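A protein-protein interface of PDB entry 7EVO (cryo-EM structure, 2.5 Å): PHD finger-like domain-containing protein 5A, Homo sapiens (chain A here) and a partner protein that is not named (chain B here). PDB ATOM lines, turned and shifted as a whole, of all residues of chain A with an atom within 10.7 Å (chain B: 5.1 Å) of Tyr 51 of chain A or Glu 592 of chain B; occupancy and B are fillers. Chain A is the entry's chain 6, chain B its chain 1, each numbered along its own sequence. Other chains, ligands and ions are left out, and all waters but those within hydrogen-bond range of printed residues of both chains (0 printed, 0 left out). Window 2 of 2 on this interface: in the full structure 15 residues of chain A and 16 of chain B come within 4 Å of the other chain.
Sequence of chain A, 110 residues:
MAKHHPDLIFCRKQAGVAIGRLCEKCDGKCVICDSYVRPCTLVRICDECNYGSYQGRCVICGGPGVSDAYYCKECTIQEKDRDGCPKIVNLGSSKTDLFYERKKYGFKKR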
ATOM      1  N   ALA A  18      16.890 -14.227  19.111  1.00  0.00           N
ATOM      2  CA  ALA A  18      17.208 -13.854  20.481  1.00  0.00           C
ATOM      3  C   ALA A  18      17.991 -12.547  20.521  1.00  0.00           C
ATOM      4  O   ALA A  18      18.879 -12.312  19.700  1.00  0.00           O
ATOM      5  CB  ALA A  18      18.005 -14.962  21.166  1.00  0.00           C
ATOM      6  N   ILE A  19      17.653 -11.699  21.489  1.00  0.00           N
ATOM      7  CA  ILE A  19      18.278 -10.393  21.663  1.00  0.00           C
ATOM      8  C   ILE A  19      19.444 -10.526  22.631  1.00  0.00           C
ATOM      9  O   ILE A  19      19.343 -11.216  23.652  1.00  0.00           O
ATOM     10  CB  ILE A  19      17.257  -9.355  22.170  1.00  0.00           C
ATOM     11  CG1 ILE A  19      15.996  -9.367  21.303  1.00  0.00           C
ATOM     12  CG2 ILE A  19      17.872  -7.969  22.200  1.00  0.00           C
ATOM     13  CD1 ILE A  19      16.248  -9.081  19.849  1.00  0.00           C
ATOM     14  N   ILE A  45      21.742 -12.886  18.767  1.00  0.00           N
ATOM     15  CA  ILE A  45      22.620 -14.002  19.086  1.00  0.00           C
ATOM     16  C   ILE A  45      21.984 -15.292  18.588  1.00  0.00           C
ATOM     17  O   ILE A  45      20.785 -15.361  18.318  1.00  0.00           O
ATOM     18  CB  ILE A  45      22.931 -14.094  20.593  1.00  0.00           C
ATOM     19  CG1 ILE A  45      21.641 -14.106  21.412  1.00  0.00           C
ATOM     20  CG2 ILE A  45      23.831 -12.948  21.020  1.00  0.00           C
ATOM     21  CD1 ILE A  45      21.793 -14.745  22.760  1.00  0.00           C
ATOM     22  N   CYS A  46      22.816 -16.325  18.471  1.00  0.00           N
ATOM     23  CA  CYS A  46      22.374 -17.622  17.985  1.00  0.00           C
ATOM     24  C   CYS A  46      21.602 -18.367  19.074  1.00  0.00           C
ATOM     25  O   CYS A  46      21.444 -17.898  20.203  1.00  0.00           O
ATOM     26  CB  CYS A  46      23.572 -18.432  17.495  1.00  0.00           C
ATOM     27  SG  CYS A  46      24.709 -18.964  18.788  1.00  0.00           S
ATOM     28  N   ASP A  47      21.111 -19.556  18.721  1.00  0.00           N
ATOM     29  CA  ASP A  47      20.293 -20.354  19.623  1.00  0.00           C
ATOM     30  C   ASP A  47      21.092 -21.136  20.655  1.00  0.00           C
ATOM     31  O   ASP A  47      20.547 -21.449  21.718  1.00  0.00           O
ATOM     32  CB  ASP A  47      19.420 -21.332  18.825  1.00  0.00           C
ATOM     33  CG  ASP A  47      18.260 -20.648  18.131  1.00  0.00           C
ATOM     34  OD1 ASP A  47      17.795 -19.603  18.626  1.00  0.00           O
ATOM     35  OD2 ASP A  47      17.808 -21.163  17.088  1.00  0.00           O
ATOM     36  N   GLU A  48      22.355 -21.469  20.381  1.00  0.00           N
ATOM     37  CA  GLU A  48      23.141 -22.181  21.382  1.00  0.00           C
ATOM     38  C   GLU A  48      23.665 -21.228  22.449  1.00  0.00           C
ATOM     39  O   GLU A  48      23.972 -21.655  23.568  1.00  0.00           O
ATOM     40  CB  GLU A  48      24.286 -22.953  20.719  1.00  0.00           C
ATOM     41  CG  GLU A  48      25.417 -22.104  20.159  1.00  0.00           C
ATOM     42  CD  GLU A  48      26.601 -21.988  21.108  1.00  0.00           C
ATOM     43  OE1 GLU A  48      27.080 -20.857  21.330  1.00  0.00           O
ATOM     44  OE2 GLU A  48      27.056 -23.028  21.628  1.00  0.00           O
ATOM     45  N   CYS A  49      23.770 -19.938  22.126  1.00  0.00           N
ATOM     46  CA  CYS A  49      24.110 -18.933  23.123  1.00  0.00           C
ATOM     47  C   CYS A  49      22.917 -18.538  23.982  1.00  0.00           C
ATOM     48  O   CYS A  49      23.106 -17.960  25.056  1.00  0.00           O
ATOM     49  CB  CYS A  49      24.682 -17.684  22.447  1.00  0.00           C
ATOM     50  SG  CYS A  49      26.349 -17.876  21.772  1.00  0.00           S
ATOM     51  N   ASN A  50      21.700 -18.828  23.530  1.00  0.00           N
ATOM     52  CA  ASN A  50      20.477 -18.499  24.258  1.00  0.00           C
ATOM     53  C   ASN A  50      19.751 -19.810  24.539  1.00  0.00           C
ATOM     54  O   ASN A  50      18.859 -20.216  23.796  1.00  0.00           O
ATOM     55  CB  ASN A  50      19.615 -17.545  23.436  1.00  0.00           C
ATOM     56  CG  ASN A  50      18.568 -16.834  24.261  1.00  0.00           C
ATOM     57  OD1 ASN A  50      18.892 -16.031  25.131  1.00  0.00           O
ATOM     58  ND2 ASN A  50      17.302 -17.120  23.990  1.00  0.00           N
ATOM     59  N   TYR A  51      20.129 -20.475  25.628  1.00  0.00           N
ATOM     60  CA  TYR A  51      19.520 -21.758  25.946  1.00  0.00           C
ATOM     61  C   TYR A  51      19.773 -22.105  27.405  1.00  0.00           C
ATOM     62  O   TYR A  51      20.908 -22.024  27.878  1.00  0.00           O
ATOM     63  CB  TYR A  51      20.059 -22.872  25.040  1.00  0.00           C
ATOM     64  CG  TYR A  51      19.461 -24.227  25.331  1.00  0.00           C
ATOM     65  CD1 TYR A  51      18.269 -24.622  24.742  1.00  0.00           C
ATOM     66  CD2 TYR A  51      20.083 -25.111  26.203  1.00  0.00           C
ATOM     67  CE1 TYR A  51      17.714 -25.858  25.009  1.00  0.00           C
ATOM     68  CE2 TYR A  51      19.536 -26.346  26.477  1.00  0.00           C
ATOM     69  CZ  TYR A  51      18.353 -26.717  25.877  1.00  0.00           C
ATOM     70  OH  TYR A  51      17.807 -27.950  26.148  1.00  0.00           O
ATOM     71  N   GLY A  52      18.711 -22.504  28.098  1.00  0.00           N
ATOM     72  CA  GLY A  52      18.844 -23.018  29.452  1.00  0.00           C
ATOM     73  C   GLY A  52      19.437 -21.991  30.393  1.00  0.00           C
ATOM     74  O   GLY A  52      18.867 -20.919  30.627  1.00  0.00           O
ATOM     75  N   SER A  53      20.609 -22.317  30.944  1.00  0.00           N
ATOM     76  CA  SER A  53      21.269 -21.409  31.875  1.00  0.00           C
ATOM     77  C   SER A  53      21.864 -20.206  31.160  1.00  0.00           C
ATOM     78  O   SER A  53      22.160 -19.189  31.797  1.00  0.00           O
ATOM     79  CB  SER A  53      22.356 -22.155  32.647  1.00  0.00           C
ATOM     80  OG  SER A  53      21.969 -23.490  32.911  1.00  0.00           O
ATOM     81  N   TYR A  54      22.051 -20.300  29.846  1.00  0.00           N
ATOM     82  CA  TYR A  54      22.624 -19.221  29.057  1.00  0.00           C
ATOM     83  C   TYR A  54      21.583 -18.214  28.586  1.00  0.00           C
ATOM     84  O   TYR A  54      21.904 -17.363  27.751  1.00  0.00           O
ATOM     85  CB  TYR A  54      23.363 -19.787  27.839  1.00  0.00           C
ATOM     86  CG  TYR A  54      24.392 -20.853  28.146  1.00  0.00           C
ATOM     87  CD1 TYR A  54      25.064 -20.880  29.360  1.00  0.00           C
ATOM     88  CD2 TYR A  54      24.704 -21.826  27.205  1.00  0.00           C
ATOM     89  CE1 TYR A  54      26.007 -21.850  29.634  1.00  0.00           C
ATOM     90  CE2 TYR A  54      25.646 -22.797  27.468  1.00  0.00           C
ATOM     91  CZ  TYR A  54      26.293 -22.806  28.683  1.00  0.00           C
ATOM     92  OH  TYR A  54      27.231 -23.776  28.949  1.00  0.00           O
ATOM     93  N   GLN A  55      20.354 -18.286  29.100  1.00  0.00           N
ATOM     94  CA  GLN A  55      19.258 -17.511  28.523  1.00  0.00           C
ATOM     95  C   GLN A  55      19.507 -16.011  28.636  1.00  0.00           C
ATOM     96  O   GLN A  55      19.435 -15.282  27.641  1.00  0.00           O
ATOM     97  CB  GLN A  55      17.939 -17.887  29.195  1.00  0.00           C
ATOM     98  CG  GLN A  55      16.727 -17.581  28.341  1.00  0.00           C
ATOM     99  CD  GLN A  55      16.140 -16.216  28.629  1.00  0.00           C
ATOM    100  OE1 GLN A  55      16.142 -15.753  29.769  1.00  0.00           O
ATOM    101  NE2 GLN A  55      15.637 -15.560  27.590  1.00  0.00           N
ATOM    102  N   GLY A  56      19.797 -15.527  29.837  1.00  0.00           N
ATOM    103  CA  GLY A  56      20.091 -14.116  29.991  1.00  0.00           C
ATOM    104  C   GLY A  56      21.482 -13.892  30.537  1.00  0.00           C
ATOM    105  O   GLY A  56      21.744 -14.153  31.715  1.00  0.00           O
ATOM    106  N   ARG A  57      22.382 -13.389  29.696  1.00  0.00           N
ATOM    107  CA  ARG A  57      23.781 -13.275  30.077  1.00  0.00           C
ATOM    108  C   ARG A  57      24.429 -12.176  29.253  1.00  0.00           C
ATOM    109  O   ARG A  57      24.060 -11.965  28.097  1.00  0.00           O
ATOM    110  CB  ARG A  57      24.524 -14.599  29.861  1.00  0.00           C
ATOM    111  CG  ARG A  57      24.452 -15.562  31.030  1.00  0.00           C
ATOM    112  CD  ARG A  57      25.490 -16.655  30.899  1.00  0.00           C
ATOM    113  NE  ARG A  57      25.407 -17.329  29.608  1.00  0.00           N
ATOM    114  CZ  ARG A  57      26.461 -17.780  28.938  1.00  0.00           C
ATOM    115  NH1 ARG A  57      26.300 -18.381  27.768  1.00  0.00           N
ATOM    116  NH2 ARG A  57      27.680 -17.630  29.437  1.00  0.00           N
ATOM    117  N   CYS A  85      27.060 -14.616  15.290  1.00  0.00           N
ATOM    118  CA  CYS A  85      26.797 -14.278  16.681  1.00  0.00           C
ATOM    119  C   CYS A  85      28.022 -13.602  17.289  1.00  0.00           C
ATOM    120  O   CYS A  85      29.126 -14.154  17.221  1.00  0.00           O
ATOM    121  CB  CYS A  85      26.431 -15.536  17.465  1.00  0.00           C
ATOM    122  SG  CYS A  85      26.080 -15.277  19.216  1.00  0.00           S
ATOM    123  N   LYS A  87      28.763 -13.120  20.440  1.00  0.00           N
ATOM    124  CA  LYS A  87      29.014 -13.488  21.828  1.00  0.00           C
ATOM    125  C   LYS A  87      30.479 -13.859  22.021  1.00  0.00           C
ATOM    126  O   LYS A  87      31.032 -14.648  21.249  1.00  0.00           O
ATOM    127  CB  LYS A  87      28.113 -14.650  22.233  1.00  0.00           C
ATOM    128  CG  LYS A  87      27.626 -14.577  23.657  1.00  0.00           C
ATOM    129  CD  LYS A  87      28.358 -15.579  24.523  1.00  0.00           C
ATOM    130  CE  LYS A  87      27.560 -15.926  25.766  1.00  0.00           C
ATOM    131  NZ  LYS A  87      28.413 -16.623  26.764  1.00  0.00           N
ATOM    132  N   ASP B 546      22.878 -28.851  33.779  1.00  0.00           N
ATOM    133  CA  ASP B 546      21.939 -28.519  32.712  1.00  0.00           C
ATOM    134  C   ASP B 546      22.585 -28.678  31.341  1.00  0.00           C
ATOM    135  O   ASP B 546      22.035 -29.353  30.460  1.00  0.00           O
ATOM    136  CB  ASP B 546      21.416 -27.095  32.898  1.00  0.00           C
ATOM    137  CG  ASP B 546      21.084 -26.779  34.345  1.00  0.00           C
ATOM    138  OD1 ASP B 546      19.915 -26.442  34.631  1.00  0.00           O
ATOM    139  OD2 ASP B 546      21.995 -26.860  35.197  1.00  0.00           O
ATOM    140  N   GLN B 547      23.758 -28.076  31.143  1.00  0.00           N
ATOM    141  CA  GLN B 547      24.387 -28.123  29.829  1.00  0.00           C
ATOM    142  C   GLN B 547      25.082 -29.456  29.585  1.00  0.00           C
ATOM    143  O   GLN B 547      25.198 -29.886  28.432  1.00  0.00           O
ATOM    144  CB  GLN B 547      25.361 -26.960  29.673  1.00  0.00           C
ATOM    145  CG  GLN B 547      24.745 -25.624  30.049  1.00  0.00           C
ATOM    146  CD  GLN B 547      23.837 -25.072  28.964  1.00  0.00           C
ATOM    147  OE1 GLN B 547      23.827 -25.563  27.836  1.00  0.00           O
ATOM    148  NE2 GLN B 547      23.065 -24.046  29.304  1.00  0.00           N
ATOM    149  N   ARG B 549      23.596 -32.137  30.517  1.00  0.00           N
ATOM    150  CA  ARG B 549      22.410 -32.827  30.023  1.00  0.00           C
ATOM    151  C   ARG B 549      22.137 -32.478  28.567  1.00  0.00           C
ATOM    152  O   ARG B 549      21.768 -33.349  27.773  1.00  0.00           O
ATOM    153  CB  ARG B 549      21.203 -32.477  30.893  1.00  0.00           C
ATOM    154  CG  ARG B 549      20.138 -33.555  30.952  1.00  0.00           C
ATOM    155  CD  ARG B 549      19.008 -33.141  31.876  1.00  0.00           C
ATOM    156  NE  ARG B 549      18.624 -31.751  31.650  1.00  0.00           N
ATOM    157  CZ  ARG B 549      17.815 -31.057  32.443  1.00  0.00           C
ATOM    158  NH1 ARG B 549      17.293 -31.623  33.523  1.00  0.00           N
ATOM    159  NH2 ARG B 549      17.524 -29.797  32.153  1.00  0.00           N
ATOM    160  N   HIS B 550      22.298 -31.204  28.202  1.00  0.00           N
ATOM    161  CA  HIS B 550      22.074 -30.788  26.818  1.00  0.00           C
ATOM    162  C   HIS B 550      23.034 -31.497  25.866  1.00  0.00           C
ATOM    163  O   HIS B 550      22.629 -31.998  24.807  1.00  0.00           O
ATOM    164  CB  HIS B 550      22.220 -29.270  26.709  1.00  0.00           C
ATOM    165  CG  HIS B 550      21.746 -28.706  25.406  1.00  0.00           C
ATOM    166  ND1 HIS B 550      20.704 -29.253  24.692  1.00  0.00           N
ATOM    167  CD2 HIS B 550      22.173 -27.638  24.692  1.00  0.00           C
ATOM    168  CE1 HIS B 550      20.508 -28.548  23.591  1.00  0.00           C
ATOM    169  NE2 HIS B 550      21.387 -27.563  23.567  1.00  0.00           N
ATOM    170  N   VAL B 553      22.049 -35.071  25.486  1.00  0.00           N
ATOM    171  CA  VAL B 553      20.891 -35.212  24.608  1.00  0.00           C
ATOM    172  C   VAL B 553      21.312 -35.097  23.149  1.00  0.00           C
ATOM    173  O   VAL B 553      20.804 -35.817  22.282  1.00  0.00           O
ATOM    174  CB  VAL B 553      19.808 -34.179  24.973  1.00  0.00           C
ATOM    175  CG1 VAL B 553      18.716 -34.147  23.916  1.00  0.00           C
ATOM    176  CG2 VAL B 553      19.209 -34.500  26.333  1.00  0.00           C
ATOM    177  N   TYR B 588      13.206 -26.876  30.601  1.00  0.00           N
ATOM    178  CA  TYR B 588      14.220 -27.374  29.680  1.00  0.00           C
ATOM    179  C   TYR B 588      14.390 -28.881  29.804  1.00  0.00           C
ATOM    180  O   TYR B 588      14.715 -29.555  28.821  1.00  0.00           O
ATOM    181  CB  TYR B 588      15.543 -26.654  29.925  1.00  0.00           C
ATOM    182  CG  TYR B 588      15.479 -25.180  29.605  1.00  0.00           C
ATOM    183  CD1 TYR B 588      15.455 -24.737  28.290  1.00  0.00           C
ATOM    184  CD2 TYR B 588      15.430 -24.231  30.616  1.00  0.00           C
ATOM    185  CE1 TYR B 588      15.393 -23.390  27.991  1.00  0.00           C
ATOM    186  CE2 TYR B 588      15.370 -22.882  30.329  1.00  0.00           C
ATOM    187  CZ  TYR B 588      15.351 -22.467  29.015  1.00  0.00           C
ATOM    188  OH  TYR B 588      15.289 -21.125  28.725  1.00  0.00           O
ATOM    189  N   ALA B 589      14.167 -29.425  31.001  1.00  0.00           N
ATOM    190  CA  ALA B 589      14.099 -30.874  31.149  1.00  0.00           C
ATOM    191  C   ALA B 589      12.996 -31.459  30.276  1.00  0.00           C
ATOM    192  O   ALA B 589      13.186 -32.498  29.631  1.00  0.00           O
ATOM    193  CB  ALA B 589      13.877 -31.235  32.617  1.00  0.00           C
ATOM    194  N   ARG B 590      11.842 -30.791  30.229  1.00  0.00           N
ATOM    195  CA  ARG B 590      10.739 -31.256  29.393  1.00  0.00           C
ATOM    196  C   ARG B 590      11.100 -31.169  27.916  1.00  0.00           C
ATOM    197  O   ARG B 590      10.811 -32.088  27.140  1.00  0.00           O
ATOM    198  CB  ARG B 590       9.481 -30.441  29.693  1.00  0.00           C
ATOM    199  CG  ARG B 590       8.907 -30.674  31.079  1.00  0.00           C
ATOM    200  CD  ARG B 590       7.478 -30.167  31.176  1.00  0.00           C
ATOM    201  NE  ARG B 590       7.407 -28.717  31.023  1.00  0.00           N
ATOM    202  CZ  ARG B 590       7.283 -27.865  32.035  1.00  0.00           C
ATOM    203  NH1 ARG B 590       7.227 -26.561  31.805  1.00  0.00           N
ATOM    204  NH2 ARG B 590       7.214 -28.317  33.280  1.00  0.00           N
ATOM    205  N   VAL B 591      11.727 -30.063  27.507  1.00  0.00           N
ATOM    206  CA  VAL B 591      12.147 -29.929  26.113  1.00  0.00           C
ATOM    207  C   VAL B 591      13.127 -31.035  25.738  1.00  0.00           C
ATOM    208  O   VAL B 591      13.021 -31.639  24.663  1.00  0.00           O
ATOM    209  CB  VAL B 591      12.749 -28.534  25.860  1.00  0.00           C
ATOM    210  CG1 VAL B 591      13.074 -28.363  24.386  1.00  0.00           C
ATOM    211  CG2 VAL B 591      11.787 -27.451  26.309  1.00  0.00           C
ATOM    212  N   GLU B 592      14.089 -31.325  26.618  1.00  0.00           N
ATOM    213  CA  GLU B 592      15.081 -32.353  26.321  1.00  0.00           C
ATOM    214  C   GLU B 592      14.445 -33.735  26.249  1.00  0.00           C
ATOM    215  O   GLU B 592      14.771 -34.529  25.357  1.00  0.00           O
ATOM    216  CB  GLU B 592      16.194 -32.323  27.370  1.00  0.00           C
ATOM    217  CG  GLU B 592      17.335 -31.379  27.030  1.00  0.00           C
ATOM    218  CD  GLU B 592      17.780 -30.546  28.215  1.00  0.00           C
ATOM    219  OE1 GLU B 592      18.024 -31.125  29.293  1.00  0.00           O
ATOM    220  OE2 GLU B 592      17.888 -29.311  28.067  1.00  0.00           O
ATOM    221  N   GLY B 593      13.534 -34.043  27.177  1.00  0.00           N
ATOM    222  CA  GLY B 593      12.843 -35.320  27.119  1.00  0.00           C
ATOM    223  C   GLY B 593      12.019 -35.480  25.856  1.00  0.00           C
ATOM    224  O   GLY B 593      12.003 -36.551  25.242  1.00  0.00           O
ATOM    225  N   ARG B 594      11.335 -34.411  25.441  1.00  0.00           N
ATOM    226  CA  ARG B 594      10.529 -34.483  24.228  1.00  0.00           C
ATOM    227  C   ARG B 594      11.405 -34.643  22.993  1.00  0.00           C
ATOM    228  O   ARG B 594      11.059 -35.389  22.072  1.00  0.00           O
ATOM    229  CB  ARG B 594       9.642 -33.244  24.116  1.00  0.00           C
ATOM    230  CG  ARG B 594       8.490 -33.244  25.107  1.00  0.00           C
ATOM    231  CD  ARG B 594       7.410 -32.256  24.719  1.00  0.00           C
ATOM    232  NE  ARG B 594       7.024 -31.414  25.847  1.00  0.00           N
ATOM    233  CZ  ARG B 594       7.455 -30.171  26.036  1.00  0.00           C
ATOM    234  NH1 ARG B 594       8.288 -29.616  25.168  1.00  0.00           N
ATOM    235  NH2 ARG B 594       7.050 -29.484  27.093  1.00  0.00           N
ATOM    236  N   GLU B 595      12.557 -33.967  22.963  1.00  0.00           N
ATOM    237  CA  GLU B 595      13.481 -34.142  21.845  1.00  0.00           C
ATOM    238  C   GLU B 595      14.015 -35.568  21.785  1.00  0.00           C
ATOM    239  O   GLU B 595      14.112 -36.160  20.702  1.00  0.00           O
ATOM    240  CB  GLU B 595      14.629 -33.141  21.956  1.00  0.00           C
ATOM    241  CG  GLU B 595      15.681 -33.288  20.873  1.00  0.00           C
ATOM    242  CD  GLU B 595      16.768 -32.239  20.968  1.00  0.00           C
ATOM    243  OE1 GLU B 595      17.067 -31.792  22.096  1.00  0.00           O
ATOM    244  OE2 GLU B 595      17.327 -31.861  19.916  1.00  0.00           O
ATOM    245  N   ILE B 596      14.358 -36.137  22.943  1.00  0.00           N
ATOM    246  CA  ILE B 596      14.856 -37.510  22.981  1.00  0.00           C
ATOM    247  C   ILE B 596      13.792 -38.474  22.473  1.00  0.00           C
ATOM    248  O   ILE B 596      14.070 -39.357  21.654  1.00  0.00           O
ATOM    249  CB  ILE B 596      15.323 -37.877  24.400  1.00  0.00           C
ATOM    250  CG1 ILE B 596      16.617 -37.138  24.746  1.00  0.00           C
ATOM    251  CG2 ILE B 596      15.516 -39.379  24.528  1.00  0.00           C
ATOM    252  CD1 ILE B 596      17.233 -37.572  26.058  1.00  0.00           C
ATOM    253  N   ILE B 597      12.556 -38.322  22.954  1.00  0.00           N
ATOM    254  CA  ILE B 597      11.489 -39.226  22.530  1.00  0.00           C
ATOM    255  C   ILE B 597      11.186 -39.047  21.046  1.00  0.00           C
ATOM    256  O   ILE B 597      10.874 -40.014  20.343  1.00  0.00           O
ATOM    257  CB  ILE B 597      10.238 -39.023  23.402  1.00  0.00           C
ATOM    258  CG1 ILE B 597      10.525 -39.451  24.841  1.00  0.00           C
ATOM    259  CG2 ILE B 597       9.061 -39.814  22.852  1.00  0.00           C
ATOM    260  CD1 ILE B 597       9.303 -39.489  25.720  1.00  0.00           C
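The backbone carbonyl oxygen (O) of Tyr 51 of chain A is in hydrogen-bond range of the side-chain amide nitrogen (NE2) of Gln 547 of chain B. The side-chain amide nitrogen (NE2) of Gln 547 of chain B lies close to the backbone NH (N) of Ser 53 of chain A. A ring nitrogen (ND1) of His 550 of chain B lies within hydrogen-bond range of the side-chain hydroxyl (OH) of Tyr 51 of chain A (3.5 Å). OH of Tyr 51 of chain A lies close to OE2 of Glu 592 of chain B (2.4 Å).
NE of Arg 549 of chain B is in salt-bridge range of OE1 of Glu 592 of chain B (2.5 Å). The side-chain amide oxygen (OD1) of Asn 50 of chain A lies close to the backbone carbonyl oxygen (O) of Gln 55 of chain A (2.7 Å).
Among the printed residues, pairs that only touch across the chains: Tyr 54 of chain A with Gln 547 of chain B, Gly 52 of chain A with Tyr 588 of chain B, Ser 53 of chain A with Asp 546 of chain B and Gln 55 of chain A with Tyr 588 of chain B.
Tyr 51 of chain A touches just these residues of chain B: Gln 547 (3.3 Å), His 550 (3.4 Å) and Glu 592 (2.4 Å). Of the printed residues of chain B, Tyr 54 of chain A touches Gln 547. Printed residues of chain B within 4 Å of Gln 55 of chain A: Tyr 588 (3.8 Å). Of the printed residues of chain A, Asp 546 of chain B touches Ser 53. Of the printed residues of chain A, Gln 547 of chain B touches Tyr 51 (3.3 Å), Ser 53 (3.4 Å) and Tyr 54 (3.3 Å). No residue of chain A comes within 4 Å of Arg 549 of chain B. His 550 of chain B touches just one residue of chain A: Tyr 51. Of the printed residues of chain A, Tyr 588 of chain B touches Gly 52 and Gln 55. No residue of chain A comes within 4 Å of Ala 589 of chain B. Of chain A, only Tyr 51 (2.4 Å) comes within 4 Å of Glu 592 of chain B. No residue of chain A comes within 4 Å of Gly 593 of chain B. No residue of chain A comes within 4 Å of Ile 596 of chain B. The nearest residue of chain B that does not touch Tyr 51 of chain A is Tyr 588 of chain B (4.1 Å). The nearest residue of chain A that does not touch Glu 592 of chain B is Gly 52 of chain A (6.5 Å).
Of the 15 printed residues of chain B, 5 touch a printed residue of chain A. Hydrophobic or aromatic side chains of chain B that line the printed part of chain A: His 550 and Tyr 588. Of the 17 printed residues of chain A, 5 touch a printed residue of chain B. Among the printed residues, 8 pairs touch across the chains. Among the printed residues, no Asp or Glu carboxylate lies within 4 Å of a Lys or Arg side-chain nitrogen of the other chain.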
